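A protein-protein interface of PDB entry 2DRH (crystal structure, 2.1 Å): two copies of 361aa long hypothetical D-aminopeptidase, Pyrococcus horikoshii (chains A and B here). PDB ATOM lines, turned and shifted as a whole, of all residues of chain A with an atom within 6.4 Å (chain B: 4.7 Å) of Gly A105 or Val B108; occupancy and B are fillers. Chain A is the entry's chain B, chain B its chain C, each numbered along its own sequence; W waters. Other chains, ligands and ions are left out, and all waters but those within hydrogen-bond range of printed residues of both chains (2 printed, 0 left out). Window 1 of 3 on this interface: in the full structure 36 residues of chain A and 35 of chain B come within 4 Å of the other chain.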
ATOM      1  N   VAL A  81      12.551  13.111 -38.907  1.00  0.00           N
ATOM      2  CA  VAL A  81      13.757  13.861 -38.596  1.00  0.00           C
ATOM      3  C   VAL A  81      14.836  13.524 -39.632  1.00  0.00           C
ATOM      4  O   VAL A  81      15.046  12.359 -39.945  1.00  0.00           O
ATOM      5  CB  VAL A  81      14.276  13.507 -37.181  1.00  0.00           C
ATOM      6  CG1 VAL A  81      15.626  14.176 -36.928  1.00  0.00           C
ATOM      7  CG2 VAL A  81      13.248  13.933 -36.133  1.00  0.00           C
ATOM      8  N   THR A 101       5.650   7.909 -32.763  1.00  0.00           N
ATOM      9  CA  THR A 101       5.643   9.371 -32.834  1.00  0.00           C
ATOM     10  C   THR A 101       6.243  10.142 -31.656  1.00  0.00           C
ATOM     11  O   THR A 101       7.004  11.085 -31.864  1.00  0.00           O
ATOM     12  CB  THR A 101       4.208   9.900 -33.060  1.00  0.00           C
ATOM     13  OG1 THR A 101       3.576   9.130 -34.087  1.00  0.00           O
ATOM     14  CG2 THR A 101       4.237  11.370 -33.491  1.00  0.00           C
ATOM     15  N   LEU A 102       5.917   9.753 -30.426  1.00  0.00           N
ATOM     16  CA  LEU A 102       6.434  10.470 -29.262  1.00  0.00           C
ATOM     17  C   LEU A 102       7.841  10.082 -28.798  1.00  0.00           C
ATOM     18  O   LEU A 102       8.361  10.663 -27.837  1.00  0.00           O
ATOM     19  CB  LEU A 102       5.448  10.360 -28.090  1.00  0.00           C
ATOM     20  CG  LEU A 102       4.380  11.461 -28.051  1.00  0.00           C
ATOM     21  CD1 LEU A 102       3.716  11.551 -29.392  1.00  0.00           C
ATOM     22  CD2 LEU A 102       3.341  11.184 -26.968  1.00  0.00           C
ATOM     23  N   SER A 103       8.465   9.130 -29.484  1.00  0.00           N
ATOM     24  CA  SER A 103       9.819   8.704 -29.116  1.00  0.00           C
ATOM     25  C   SER A 103      10.899   9.116 -30.115  1.00  0.00           C
ATOM     26  O   SER A 103      12.022   8.613 -30.059  1.00  0.00           O
ATOM     27  CB  SER A 103       9.868   7.184 -28.928  1.00  0.00           C
ATOM     28  OG  SER A 103       9.106   6.774 -27.803  1.00  0.00           O
ATOM     29  N   ILE A 104      10.571  10.030 -31.027  1.00  0.00           N
ATOM     30  CA  ILE A 104      11.553  10.472 -32.012  1.00  0.00           C
ATOM     31  C   ILE A 104      12.696  11.191 -31.316  1.00  0.00           C
ATOM     32  O   ILE A 104      13.860  11.043 -31.702  1.00  0.00           O
ATOM     33  CB  ILE A 104      10.933  11.411 -33.074  1.00  0.00           C
ATOM     34  CG1 ILE A 104      10.277  12.614 -32.395  1.00  0.00           C
ATOM     35  CG2 ILE A 104       9.930  10.632 -33.922  1.00  0.00           C
ATOM     36  CD1 ILE A 104       9.890  13.734 -33.352  1.00  0.00           C
ATOM     37  N   GLY A 105      12.360  11.970 -30.288  1.00  0.00           N
ATOM     38  CA  GLY A 105      13.383  12.679 -29.542  1.00  0.00           C
ATOM     39  C   GLY A 105      14.332  11.663 -28.940  1.00  0.00           C
ATOM     40  O   GLY A 105      15.553  11.746 -29.109  1.00  0.00           O
ATOM     41  N   THR A 106      13.764  10.680 -28.248  1.00  0.00           N
ATOM     42  CA  THR A 106      14.551   9.636 -27.613  1.00  0.00           C
ATOM     43  C   THR A 106      15.379   8.889 -28.654  1.00  0.00           C
ATOM     44  O   THR A 106      16.533   8.532 -28.415  1.00  0.00           O
ATOM     45  CB  THR A 106      13.632   8.637 -26.887  1.00  0.00           C
ATOM     46  OG1 THR A 106      12.674   9.358 -26.096  1.00  0.00           O
ATOM     47  CG2 THR A 106      14.447   7.725 -25.977  1.00  0.00           C
ATOM     48  N   ALA A 107      14.771   8.653 -29.812  1.00  0.00           N
ATOM     49  CA  ALA A 107      15.423   7.948 -30.902  1.00  0.00           C
ATOM     50  C   ALA A 107      16.668   8.708 -31.356  1.00  0.00           C
ATOM     51  O   ALA A 107      17.732   8.111 -31.544  1.00  0.00           O
ATOM     52  CB  ALA A 107      14.450   7.772 -32.063  1.00  0.00           C
ATOM     53  N   VAL A 108      16.527  10.019 -31.533  1.00  0.00           N
ATOM     54  CA  VAL A 108      17.643  10.870 -31.940  1.00  0.00           C
ATOM     55  C   VAL A 108      18.770  10.800 -30.899  1.00  0.00           C
ATOM     56  O   VAL A 108      19.956  10.766 -31.248  1.00  0.00           O
ATOM     57  CB  VAL A 108      17.192  12.346 -32.099  1.00  0.00           C
ATOM     58  CG1 VAL A 108      18.404  13.257 -32.266  1.00  0.00           C
ATOM     59  CG2 VAL A 108      16.278  12.478 -33.302  1.00  0.00           C
ATOM     60  N   GLU A 109      18.392  10.781 -29.624  1.00  0.00           N
ATOM     61  CA  GLU A 109      19.371  10.698 -28.541  1.00  0.00           C
ATOM     62  C   GLU A 109      20.132   9.379 -28.627  1.00  0.00           C
ATOM     63  O   GLU A 109      21.354   9.343 -28.468  1.00  0.00           O
ATOM     64  CB  GLU A 109      18.672  10.809 -27.186  1.00  0.00           C
ATOM     65  CG  GLU A 109      18.165  12.214 -26.871  1.00  0.00           C
ATOM     66  CD  GLU A 109      19.284  13.166 -26.469  1.00  0.00           C
ATOM     67  OE1 GLU A 109      20.316  13.237 -27.177  1.00  0.00           O
ATOM     68  OE2 GLU A 109      19.128  13.853 -25.439  1.00  0.00           O
ATOM     69  N   GLY A 110      19.399   8.297 -28.892  1.00  0.00           N
ATOM     70  CA  GLY A 110      20.023   6.994 -28.994  1.00  0.00           C
ATOM     71  C   GLY A 110      20.852   6.851 -30.251  1.00  0.00           C
ATOM     72  O   GLY A 110      21.958   6.306 -30.219  1.00  0.00           O
ATOM     73  N   VAL A 133      15.272   9.733 -38.614  1.00  0.00           N
ATOM     74  CA  VAL A 133      14.271   9.067 -37.797  1.00  0.00           C
ATOM     75  C   VAL A 133      12.862   9.325 -38.335  1.00  0.00           C
ATOM     76  O   VAL A 133      12.479  10.469 -38.548  1.00  0.00           O
ATOM     77  CB  VAL A 133      14.335   9.588 -36.347  1.00  0.00           C
ATOM     78  CG1 VAL A 133      13.296   8.878 -35.482  1.00  0.00           C
ATOM     79  CG2 VAL A 133      15.743   9.400 -35.782  1.00  0.00           C
ATOM     80  N   ARG A 147       6.343   7.240 -23.396  1.00  0.00           N
ATOM     81  CA  ARG A 147       7.681   7.274 -23.987  1.00  0.00           C
ATOM     82  C   ARG A 147       8.541   6.181 -23.373  1.00  0.00           C
ATOM     83  O   ARG A 147       9.550   6.451 -22.726  1.00  0.00           O
ATOM     84  CB  ARG A 147       8.330   8.648 -23.777  1.00  0.00           C
ATOM     85  CG  ARG A 147       7.889   9.688 -24.802  1.00  0.00           C
ATOM     86  CD  ARG A 147       8.602  11.022 -24.630  1.00  0.00           C
ATOM     87  NE  ARG A 147       8.051  11.808 -23.531  1.00  0.00           N
ATOM     88  CZ  ARG A 147       8.524  12.990 -23.148  1.00  0.00           C
ATOM     89  NH1 ARG A 147       9.566  13.530 -23.769  1.00  0.00           N
ATOM     90  NH2 ARG A 147       7.944  13.641 -22.152  1.00  0.00           N
ATOM     91  N   VAL B  81      13.456  19.953 -37.081  1.00  0.00           N
ATOM     92  CA  VAL B  81      12.429  19.003 -36.682  1.00  0.00           C
ATOM     93  C   VAL B  81      11.048  19.659 -36.774  1.00  0.00           C
ATOM     94  O   VAL B  81      10.842  20.759 -36.256  1.00  0.00           O
ATOM     95  CB  VAL B  81      12.667  18.518 -35.232  1.00  0.00           C
ATOM     96  CG1 VAL B  81      11.509  17.629 -34.765  1.00  0.00           C
ATOM     97  CG2 VAL B  81      13.990  17.753 -35.167  1.00  0.00           C
ATOM     98  N   ILE B 104      19.044  18.607 -30.620  1.00  0.00           N
ATOM     99  CA  ILE B 104      17.667  18.617 -31.113  1.00  0.00           C
ATOM    100  C   ILE B 104      16.866  17.501 -30.444  1.00  0.00           C
ATOM    101  O   ILE B 104      15.692  17.677 -30.113  1.00  0.00           O
ATOM    102  CB  ILE B 104      17.587  18.423 -32.646  1.00  0.00           C
ATOM    103  CG1 ILE B 104      18.389  17.192 -33.062  1.00  0.00           C
ATOM    104  CG2 ILE B 104      18.087  19.677 -33.358  1.00  0.00           C
ATOM    105  CD1 ILE B 104      18.142  16.769 -34.501  1.00  0.00           C
ATOM    106  N   GLY B 105      17.514  16.357 -30.242  1.00  0.00           N
ATOM    107  CA  GLY B 105      16.852  15.234 -29.605  1.00  0.00           C
ATOM    108  C   GLY B 105      16.381  15.628 -28.221  1.00  0.00           C
ATOM    109  O   GLY B 105      15.216  15.429 -27.868  1.00  0.00           O
ATOM    110  N   THR B 106      17.296  16.204 -27.442  1.00  0.00           N
ATOM    111  CA  THR B 106      16.997  16.643 -26.087  1.00  0.00           C
ATOM    112  C   THR B 106      15.933  17.738 -26.110  1.00  0.00           C
ATOM    113  O   THR B 106      15.061  17.795 -25.238  1.00  0.00           O
ATOM    114  CB  THR B 106      18.253  17.207 -25.405  1.00  0.00           C
ATOM    115  OG1 THR B 106      19.383  16.386 -25.728  1.00  0.00           O
ATOM    116  CG2 THR B 106      18.067  17.232 -23.894  1.00  0.00           C
ATOM    117  N   ALA B 107      16.020  18.611 -27.111  1.00  0.00           N
ATOM    118  CA  ALA B 107      15.070  19.707 -27.260  1.00  0.00           C
ATOM    119  C   ALA B 107      13.666  19.136 -27.446  1.00  0.00           C
ATOM    120  O   ALA B 107      12.705  19.610 -26.835  1.00  0.00           O
ATOM    121  CB  ALA B 107      15.459  20.586 -28.454  1.00  0.00           C
ATOM    122  N   VAL B 108      13.554  18.123 -28.301  1.00  0.00           N
ATOM    123  CA  VAL B 108      12.273  17.465 -28.551  1.00  0.00           C
ATOM    124  C   VAL B 108      11.725  16.893 -27.242  1.00  0.00           C
ATOM    125  O   VAL B 108      10.555  17.103 -26.901  1.00  0.00           O
ATOM    126  CB  VAL B 108      12.418  16.307 -29.567  1.00  0.00           C
ATOM    127  CG1 VAL B 108      11.110  15.517 -29.656  1.00  0.00           C
ATOM    128  CG2 VAL B 108      12.790  16.862 -30.943  1.00  0.00           C
ATOM    129  N   GLU B 109      12.573  16.167 -26.517  1.00  0.00           N
ATOM    130  CA  GLU B 109      12.174  15.573 -25.245  1.00  0.00           C
ATOM    131  C   GLU B 109      11.639  16.646 -24.303  1.00  0.00           C
ATOM    132  O   GLU B 109      10.564  16.486 -23.712  1.00  0.00           O
ATOM    133  CB  GLU B 109      13.369  14.869 -24.599  1.00  0.00           C
ATOM    134  CG  GLU B 109      13.815  13.622 -25.350  1.00  0.00           C
ATOM    135  CD  GLU B 109      12.886  12.445 -25.118  1.00  0.00           C
ATOM    136  OE1 GLU B 109      11.651  12.623 -25.215  1.00  0.00           O
ATOM    137  OE2 GLU B 109      13.393  11.335 -24.843  1.00  0.00           O
ATOM    138  N   GLY B 110      12.399  17.737 -24.183  1.00  0.00           N
ATOM    139  CA  GLY B 110      12.026  18.841 -23.318  1.00  0.00           C
ATOM    140  C   GLY B 110      10.751  19.527 -23.754  1.00  0.00           C
ATOM    141  O   GLY B 110       9.936  19.927 -22.917  1.00  0.00           O
ATOM    142  N   LEU B 111      10.576  19.677 -25.064  1.00  0.00           N
ATOM    143  CA  LEU B 111       9.374  20.309 -25.585  1.00  0.00           C
ATOM    144  C   LEU B 111       8.173  19.398 -25.322  1.00  0.00           C
ATOM    145  O   LEU B 111       7.104  19.862 -24.916  1.00  0.00           O
ATOM    146  CB  LEU B 111       9.522  20.581 -27.085  1.00  0.00           C
ATOM    147  CG  LEU B 111       8.404  21.370 -27.775  1.00  0.00           C
ATOM    148  CD1 LEU B 111       8.057  22.622 -26.967  1.00  0.00           C
ATOM    149  CD2 LEU B 111       8.855  21.757 -29.178  1.00  0.00           C
ATOM    150  N   LEU B 112       8.347  18.101 -25.547  1.00  0.00           N
ATOM    151  CA  LEU B 112       7.257  17.172 -25.301  1.00  0.00           C
ATOM    152  C   LEU B 112       6.867  17.183 -23.819  1.00  0.00           C
ATOM    153  O   LEU B 112       5.685  17.087 -23.485  1.00  0.00           O
ATOM    154  CB  LEU B 112       7.647  15.758 -25.741  1.00  0.00           C
ATOM    155  CG  LEU B 112       7.689  15.537 -27.258  1.00  0.00           C
ATOM    156  CD1 LEU B 112       8.088  14.105 -27.560  1.00  0.00           C
ATOM    157  CD2 LEU B 112       6.324  15.849 -27.865  1.00  0.00           C
ATOM    158  N   PRO B 131       6.449  18.673 -32.693  1.00  0.00           N
ATOM    159  CA  PRO B 131       7.369  19.638 -32.093  1.00  0.00           C
ATOM    160  C   PRO B 131       8.197  20.324 -33.168  1.00  0.00           C
ATOM    161  O   PRO B 131       8.650  19.677 -34.115  1.00  0.00           O
ATOM    162  CB  PRO B 131       8.221  18.773 -31.168  1.00  0.00           C
ATOM    163  CG  PRO B 131       8.257  17.447 -31.899  1.00  0.00           C
ATOM    164  CD  PRO B 131       6.816  17.292 -32.331  1.00  0.00           C
ATOM    165  N   VAL B 133      11.567  22.230 -33.849  1.00  0.00           N
ATOM    166  CA  VAL B 133      12.902  22.492 -33.332  1.00  0.00           C
ATOM    167  C   VAL B 133      13.886  22.771 -34.456  1.00  0.00           C
ATOM    168  O   VAL B 133      14.003  21.983 -35.394  1.00  0.00           O
ATOM    169  CB  VAL B 133      13.425  21.285 -32.530  1.00  0.00           C
ATOM    170  CG1 VAL B 133      14.836  21.564 -32.025  1.00  0.00           C
ATOM    171  CG2 VAL B 133      12.482  20.976 -31.365  1.00  0.00           C
HETATM  172  O   HOH W   1      10.982  11.703 -27.774  1.00  0.00           O
HETATM  173  O   HOH W   2      19.911  15.237 -28.891  1.00  0.00           O
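The guanidinium group of Arg A147 is in salt-bridge range of the side-chain carboxylate of Glu B109 (2.7 Å). OG1 of Thr B106 sits at hydrogen-bond distance from OE2 of Glu A109, at 2.6 Å. The side-chain hydroxyl (OG1) of Thr A106 is in hydrogen-bond range of the side-chain carboxylate (OE2) of Glu B109 (2.4 Å).
CD1 of Leu B112 touches O of Leu A102, 3.5 Å away. O of Gly B105 touches CA of Gly A105 (3.7 Å). Gly A105 touches Val B108. CG1 of Val A108 touches CA of Gly B105, 3.7 Å away. Arg A147 touches Leu B112 (NH1 to CB, 3.5 Å).
Water W2 lies within hydrogen-bond range of the side-chain carboxylate (OE1) of Glu A109 (2.7 Å), the backbone NH (N) of Gly B105 (3.0 Å) and the backbone NH (N) of Thr B106 (3.1 Å). Water W1 lies within hydrogen-bond range of the side-chain carboxylate (OE1) of Glu B109 (2.8 Å), the backbone carbonyl oxygen (O) of Leu A102 (2.8 Å), the backbone NH (N) of Gly A105 (2.9 Å) and the backbone NH (N) of Thr A106 (3.0 Å).
Hydrophobic or aromatic side chains of chain A that line the printed part of chain B: Val A108. Hydrophobic or aromatic side chains of chain B within 4 Å of the printed part of chain A: Val B108 and Leu B112. Along chain B the printed residues that touch a printed residue of chain A span positions 105 to 112. Among the printed residues, 8 pairs touch across the chains. Among the printed residues, Asp or Glu carboxylates within 4 Å of a Lys or Arg side-chain nitrogen of the other chain: Arg A147 with Glu B109.
Gly A105 touches its own counterpart, Gly B105. Gly A105 touches Val B108, and with the chains exchanged Val A108 touches Gly B105. Thr A106 touches Glu B109, and with the chains exchanged Glu A109 touches Thr B106. Of the 8 pairs that touch across the chains among the printed residues, 5 have their exchanged pair printed and touching as well.
Val A81 touches none of the printed residues of chain B. Of the printed residues of chain B, Leu A102 touches Leu B112. Gly A105 touches just these residues of chain B: Gly B105 (3.7 Å) and Val B108 (3.6 Å). Of the printed residues of chain A, Gly B105 touches Gly A105 (3.7 Å) and Val A108 (3.7 Å). Of the printed residues of chain A, Thr B106 touches Glu A109. Of chain A, only Gly A105 (3.6 Å) comes within 4 Å of Val B108. Of the printed residues of chain A, Glu B109 touches Thr A106 and Arg A147. Printed residues of chain A within 4 Å of Leu B112: Leu A102 (3.5 Å) and Arg A147 (3.5 Å). Pro B131 touches none of the printed residues of chain A. The nearest residue of chain A that does not touch Val B108 is Ile A104 (4.1 Å).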
